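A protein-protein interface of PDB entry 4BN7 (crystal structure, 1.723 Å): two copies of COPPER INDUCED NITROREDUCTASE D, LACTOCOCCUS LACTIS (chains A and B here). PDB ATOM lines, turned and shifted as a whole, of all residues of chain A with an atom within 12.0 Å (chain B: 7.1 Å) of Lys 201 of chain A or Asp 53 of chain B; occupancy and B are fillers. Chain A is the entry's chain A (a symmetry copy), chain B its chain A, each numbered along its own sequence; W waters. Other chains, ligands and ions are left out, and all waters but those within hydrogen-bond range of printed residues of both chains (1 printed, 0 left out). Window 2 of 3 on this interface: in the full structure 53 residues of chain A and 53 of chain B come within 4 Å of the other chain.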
ATOM      1  N   PHE A 197     -19.718 -24.579   7.288  1.00  0.00           N
ATOM      2  CA  PHE A 197     -20.134 -24.572   5.889  1.00  0.00           C
ATOM      3  C   PHE A 197     -19.777 -25.875   5.197  1.00  0.00           C
ATOM      4  O   PHE A 197     -18.615 -26.282   5.197  1.00  0.00           O
ATOM      5  CB  PHE A 197     -19.490 -23.425   5.107  1.00  0.00           C
ATOM      6  CG  PHE A 197     -19.628 -22.082   5.752  1.00  0.00           C
ATOM      7  CD1 PHE A 197     -20.861 -21.459   5.859  1.00  0.00           C
ATOM      8  CD2 PHE A 197     -18.507 -21.418   6.224  1.00  0.00           C
ATOM      9  CE1 PHE A 197     -20.968 -20.211   6.441  1.00  0.00           C
ATOM     10  CE2 PHE A 197     -18.607 -20.183   6.804  1.00  0.00           C
ATOM     11  CZ  PHE A 197     -19.838 -19.570   6.921  1.00  0.00           C
ATOM     12  N   ILE A 198     -20.782 -26.518   4.605  1.00  0.00           N
ATOM     13  CA  ILE A 198     -20.569 -27.677   3.749  1.00  0.00           C
ATOM     14  C   ILE A 198     -21.067 -27.333   2.358  1.00  0.00           C
ATOM     15  O   ILE A 198     -22.200 -26.884   2.201  1.00  0.00           O
ATOM     16  CB  ILE A 198     -21.361 -28.904   4.234  1.00  0.00           C
ATOM     17  CG1 ILE A 198     -20.884 -29.342   5.615  1.00  0.00           C
ATOM     18  CG2 ILE A 198     -21.231 -30.059   3.230  1.00  0.00           C
ATOM     19  CD1 ILE A 198     -21.762 -30.405   6.239  1.00  0.00           C
ATOM     20  N   VAL A 199     -20.220 -27.530   1.355  1.00  0.00           N
ATOM     21  CA  VAL A 199     -20.608 -27.298  -0.033  1.00  0.00           C
ATOM     22  C   VAL A 199     -20.641 -28.628  -0.782  1.00  0.00           C
ATOM     23  O   VAL A 199     -19.696 -29.416  -0.708  1.00  0.00           O
ATOM     24  CB  VAL A 199     -19.623 -26.335  -0.735  1.00  0.00           C
ATOM     25  CG1 VAL A 199     -20.017 -26.125  -2.187  1.00  0.00           C
ATOM     26  CG2 VAL A 199     -19.556 -25.011  -0.001  1.00  0.00           C
ATOM     27  N   ALA A 200     -21.736 -28.890  -1.493  1.00  0.00           N
ATOM     28  CA  ALA A 200     -21.864 -30.124  -2.260  1.00  0.00           C
ATOM     29  C   ALA A 200     -22.336 -29.815  -3.675  1.00  0.00           C
ATOM     30  O   ALA A 200     -23.151 -28.921  -3.882  1.00  0.00           O
ATOM     31  CB  ALA A 200     -22.830 -31.077  -1.571  1.00  0.00           C
ATOM     32  N   LYS A 201     -21.822 -30.566  -4.647  1.00  0.00           N
ATOM     33  CA  LYS A 201     -22.153 -30.342  -6.052  1.00  0.00           C
ATOM     34  C   LYS A 201     -22.925 -31.527  -6.632  1.00  0.00           C
ATOM     35  O   LYS A 201     -22.819 -32.652  -6.142  1.00  0.00           O
ATOM     36  CB  LYS A 201     -20.888 -30.087  -6.858  1.00  0.00           C
ATOM     37  N   ARG B  17     -30.045 -20.789 -14.047  1.00  0.00           N
ATOM     38  CA  ARG B  17     -28.689 -21.229 -13.731  1.00  0.00           C
ATOM     39  C   ARG B  17     -27.618 -20.438 -14.480  1.00  0.00           C
ATOM     40  O   ARG B  17     -26.496 -20.911 -14.674  1.00  0.00           O
ATOM     41  CB  ARG B  17     -28.568 -22.718 -14.029  1.00  0.00           C
ATOM     42  CG  ARG B  17     -29.575 -23.538 -13.254  1.00  0.00           C
ATOM     43  CD  ARG B  17     -29.408 -25.031 -13.459  1.00  0.00           C
ATOM     44  NE  ARG B  17     -30.284 -25.773 -12.560  1.00  0.00           N
ATOM     45  CZ  ARG B  17     -30.460 -27.090 -12.588  1.00  0.00           C
ATOM     46  NH1 ARG B  17     -29.812 -27.837 -13.474  1.00  0.00           N
ATOM     47  NH2 ARG B  17     -31.290 -27.660 -11.724  1.00  0.00           N
ATOM     48  N   ILE B  49     -24.694 -25.991   1.343  1.00  0.00           N
ATOM     49  CA  ILE B  49     -24.870 -25.274   0.084  1.00  0.00           C
ATOM     50  C   ILE B  49     -24.832 -26.286  -1.055  1.00  0.00           C
ATOM     51  O   ILE B  49     -23.807 -26.938  -1.278  1.00  0.00           O
ATOM     52  CB  ILE B  49     -23.755 -24.236  -0.121  1.00  0.00           C
ATOM     53  CG1 ILE B  49     -23.737 -23.256   1.055  1.00  0.00           C
ATOM     54  CG2 ILE B  49     -23.940 -23.498  -1.440  1.00  0.00           C
ATOM     55  CD1 ILE B  49     -22.453 -22.432   1.161  1.00  0.00           C
ATOM     56  N   LEU B  50     -25.961 -26.429  -1.743  1.00  0.00           N
ATOM     57  CA  LEU B  50     -26.119 -27.422  -2.802  1.00  0.00           C
ATOM     58  C   LEU B  50     -26.225 -26.781  -4.176  1.00  0.00           C
ATOM     59  O   LEU B  50     -27.039 -25.889  -4.385  1.00  0.00           O
ATOM     60  CB  LEU B  50     -27.393 -28.236  -2.564  1.00  0.00           C
ATOM     61  CG  LEU B  50     -27.536 -28.911  -1.205  1.00  0.00           C
ATOM     62  CD1 LEU B  50     -28.813 -29.718  -1.171  1.00  0.00           C
ATOM     63  CD2 LEU B  50     -26.329 -29.789  -0.922  1.00  0.00           C
ATOM     64  N   THR B  51     -25.410 -27.248  -5.113  1.00  0.00           N
ATOM     65  CA  THR B  51     -25.550 -26.851  -6.508  1.00  0.00           C
ATOM     66  C   THR B  51     -25.456 -28.095  -7.375  1.00  0.00           C
ATOM     67  O   THR B  51     -25.225 -29.195  -6.864  1.00  0.00           O
ATOM     68  CB  THR B  51     -24.464 -25.848  -6.938  1.00  0.00           C
ATOM     69  OG1 THR B  51     -23.181 -26.477  -6.886  1.00  0.00           O
ATOM     70  CG2 THR B  51     -24.473 -24.617  -6.041  1.00  0.00           C
ATOM     71  N   GLY B  52     -25.636 -27.925  -8.682  1.00  0.00           N
ATOM     72  CA  GLY B  52     -25.460 -29.017  -9.626  1.00  0.00           C
ATOM     73  C   GLY B  52     -26.276 -30.255  -9.294  1.00  0.00           C
ATOM     74  O   GLY B  52     -27.469 -30.163  -9.029  1.00  0.00           O
ATOM     75  N   ASP B  53     -25.627 -31.418  -9.308  1.00  0.00           N
ATOM     76  CA  ASP B  53     -26.321 -32.684  -9.093  1.00  0.00           C
ATOM     77  C   ASP B  53     -27.011 -32.728  -7.732  1.00  0.00           C
ATOM     78  O   ASP B  53     -28.063 -33.356  -7.581  1.00  0.00           O
ATOM     79  CB  ASP B  53     -25.348 -33.859  -9.203  1.00  0.00           C
ATOM     80  CG  ASP B  53     -24.820 -34.054 -10.610  1.00  0.00           C
ATOM     81  OD1 ASP B  53     -25.392 -33.473 -11.552  1.00  0.00           O
ATOM     82  OD2 ASP B  53     -23.833 -34.800 -10.773  1.00  0.00           O
ATOM     83  N   ALA B  54     -26.411 -32.072  -6.743  1.00  0.00           N
ATOM     84  CA  ALA B  54     -26.944 -32.099  -5.388  1.00  0.00           C
ATOM     85  C   ALA B  54     -28.235 -31.287  -5.321  1.00  0.00           C
ATOM     86  O   ALA B  54     -29.169 -31.644  -4.603  1.00  0.00           O
ATOM     87  CB  ALA B  54     -25.918 -31.567  -4.395  1.00  0.00           C
ATOM     88  N   GLN B  55     -28.281 -30.207  -6.092  1.00  0.00           N
ATOM     89  CA  GLN B  55     -29.482 -29.388  -6.216  1.00  0.00           C
ATOM     90  C   GLN B  55     -30.621 -30.224  -6.820  1.00  0.00           C
ATOM     91  O   GLN B  55     -31.728 -30.259  -6.279  1.00  0.00           O
ATOM     92  CB  GLN B  55     -29.173 -28.151  -7.069  1.00  0.00           C
ATOM     93  CG  GLN B  55     -30.367 -27.453  -7.711  1.00  0.00           C
ATOM     94  CD  GLN B  55     -31.214 -26.678  -6.717  1.00  0.00           C
ATOM     95  OE1 GLN B  55     -30.978 -26.722  -5.516  1.00  0.00           O
ATOM     96  NE2 GLN B  55     -32.212 -25.964  -7.221  1.00  0.00           N
ATOM     97  N   ASP B  56     -30.349 -30.917  -7.921  1.00  0.00           N
ATOM     98  CA  ASP B  56     -31.358 -31.785  -8.526  1.00  0.00           C
ATOM     99  C   ASP B  56     -31.849 -32.835  -7.532  1.00  0.00           C
ATOM    100  O   ASP B  56     -33.048 -33.102  -7.429  1.00  0.00           O
ATOM    101  CB  ASP B  56     -30.810 -32.490  -9.766  1.00  0.00           C
ATOM    102  CG  ASP B  56     -30.489 -31.535 -10.893  1.00  0.00           C
ATOM    103  OD1 ASP B  56     -30.986 -30.393 -10.866  1.00  0.00           O
ATOM    104  OD2 ASP B  56     -29.743 -31.934 -11.810  1.00  0.00           O
ATOM    105  N   LYS B  57     -30.914 -33.436  -6.806  1.00  0.00           N
ATOM    106  CA  LYS B  57     -31.243 -34.515  -5.882  1.00  0.00           C
ATOM    107  C   LYS B  57     -32.141 -34.035  -4.748  1.00  0.00           C
ATOM    108  O   LYS B  57     -33.096 -34.711  -4.388  1.00  0.00           O
ATOM    109  CB  LYS B  57     -29.967 -35.137  -5.309  1.00  0.00           C
ATOM    110  CG  LYS B  57     -30.220 -36.126  -4.170  1.00  0.00           C
ATOM    111  CD  LYS B  57     -29.687 -37.512  -4.481  1.00  0.00           C
ATOM    112  CE  LYS B  57     -28.173 -37.524  -4.593  1.00  0.00           C
ATOM    113  NZ  LYS B  57     -27.639 -38.911  -4.710  1.00  0.00           N
ATOM    114  N   LEU B  58     -31.840 -32.877  -4.173  1.00  0.00           N
ATOM    115  CA  LEU B  58     -32.670 -32.368  -3.085  1.00  0.00           C
ATOM    116  C   LEU B  58     -34.138 -32.347  -3.506  1.00  0.00           C
ATOM    117  O   LEU B  58     -35.010 -32.886  -2.822  1.00  0.00           O
ATOM    118  CB  LEU B  58     -32.233 -30.964  -2.660  1.00  0.00           C
ATOM    119  CG  LEU B  58     -33.144 -30.316  -1.608  1.00  0.00           C
ATOM    120  CD1 LEU B  58     -33.106 -31.092  -0.300  1.00  0.00           C
ATOM    121  CD2 LEU B  58     -32.779 -28.846  -1.386  1.00  0.00           C
ATOM    122  N   GLU B  61     -35.412 -36.045  -5.381  1.00  0.00           N
ATOM    123  CA  GLU B  61     -35.293 -37.299  -4.651  1.00  0.00           C
ATOM    124  C   GLU B  61     -35.637 -37.180  -3.168  1.00  0.00           C
ATOM    125  O   GLU B  61     -35.825 -38.194  -2.499  1.00  0.00           O
ATOM    126  CB  GLU B  61     -33.889 -37.885  -4.833  1.00  0.00           C
ATOM    127  CG  GLU B  61     -33.606 -38.313  -6.267  1.00  0.00           C
ATOM    128  CD  GLU B  61     -32.280 -39.020  -6.419  1.00  0.00           C
ATOM    129  OE1 GLU B  61     -31.965 -39.889  -5.578  1.00  0.00           O
ATOM    130  OE2 GLU B  61     -31.551 -38.702  -7.383  1.00  0.00           O
ATOM    131  N   TRP B 164     -26.467 -36.104   3.191  1.00  0.00           N
ATOM    132  CA  TRP B 164     -25.234 -35.321   3.278  1.00  0.00           C
ATOM    133  C   TRP B 164     -24.510 -35.517   4.613  1.00  0.00           C
ATOM    134  O   TRP B 164     -23.653 -34.719   4.995  1.00  0.00           O
ATOM    135  CB  TRP B 164     -25.522 -33.843   2.966  1.00  0.00           C
ATOM    136  CG  TRP B 164     -25.822 -33.675   1.507  1.00  0.00           C
ATOM    137  CD1 TRP B 164     -24.915 -33.654   0.490  1.00  0.00           C
ATOM    138  CD2 TRP B 164     -27.115 -33.564   0.892  1.00  0.00           C
ATOM    139  NE1 TRP B 164     -25.556 -33.535  -0.720  1.00  0.00           N
ATOM    140  CE2 TRP B 164     -26.907 -33.478  -0.502  1.00  0.00           C
ATOM    141  CE3 TRP B 164     -28.426 -33.534   1.380  1.00  0.00           C
ATOM    142  CZ2 TRP B 164     -27.958 -33.352  -1.407  1.00  0.00           C
ATOM    143  CZ3 TRP B 164     -29.469 -33.407   0.476  1.00  0.00           C
ATOM    144  CH2 TRP B 164     -29.228 -33.321  -0.901  1.00  0.00           C
HETATM  145  O   HOH W   1     -21.924 -26.347  -4.577  1.00  0.00           O
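The backbone NH (N) of Ile 49 of chain B lies within hydrogen-bond range of the backbone carbonyl oxygen (O) of Ile 198 of chain A, at 2.8 Å. N of Ala 200 of chain A lies within hydrogen-bond range of O of Ile 49 of chain B (2.9 Å). The backbone NH of Thr 51 of chain B is in hydrogen-bond range of the backbone carbonyl oxygen of Ala 200 of chain A (3.1 Å).
CA of Val 199 of chain A touches O of Ile 49 of chain B (3.5 Å). O of Ala 200 of chain A touches CA of Leu 50 of chain B, at 3.5 Å. Ala 200 of chain A touches Ala 54 of chain B. Ala 200 of chain A touches Trp 164 of chain B. Lys 201 of chain A touches Thr 51 of chain B (C to O, 3.3 Å). Asp 53 of chain B touches Lys 201 of chain A. Lys 201 of chain A touches Ala 54 of chain B (C to N, 3.5 Å).
Of the printed residues of chain B, Ile 198 of chain A touches Ile 49. Of the printed residues of chain B, Val 199 of chain A touches Ile 49 (3.5 Å). Printed residues of chain B within 4 Å of Ala 200 of chain A: Ile 49 (2.9 Å), Leu 50 (3.5 Å), Thr 51 (3.1 Å), Ala 54 (3.9 Å) and Trp 164 (3.8 Å). Of the printed residues of chain A, Ile 49 of chain B touches Ile 198, Val 199 and Ala 200. Leu 50 of chain B touches just one residue of chain A: Ala 200 (3.5 Å). Thr 51 of chain B touches just these residues of chain A: Ala 200 and Lys 201. Asp 53 of chain B touches just one residue of chain A: Lys 201 (3.8 Å). Printed residues of chain A within 4 Å of Ala 54 of chain B: Ala 200 (3.9 Å) and Lys 201 (3.5 Å). No residue of chain A comes within 4 Å of Asp 56 of chain B. No residue of chain A comes within 4 Å of Lys 57 of chain B. Of the printed residues of chain A, Trp 164 of chain B touches Ala 200. The nearest residue of chain A that does not touch Asp 53 of chain B is Ala 200 of chain A (6.5 Å). The nearest printed residue of chain B that does not touch Ile 198 of chain A is Trp 164 of chain B (4.9 Å).
Hydrophobic or aromatic side chains of chain A within 4 Å of the printed part of chain B: Val 199 and Ala 200. Among the printed residues, no Asp or Glu carboxylate lies within 4 Å of a Lys or Arg side-chain nitrogen of the other chain.
No position is printed for both chains.
Water W1 bridges the side-chain hydroxyl (OG1) of Thr 51 of chain B (2.6 Å) and the backbone carbonyl oxygen (O) of Ala 200 of chain A (2.9 Å).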
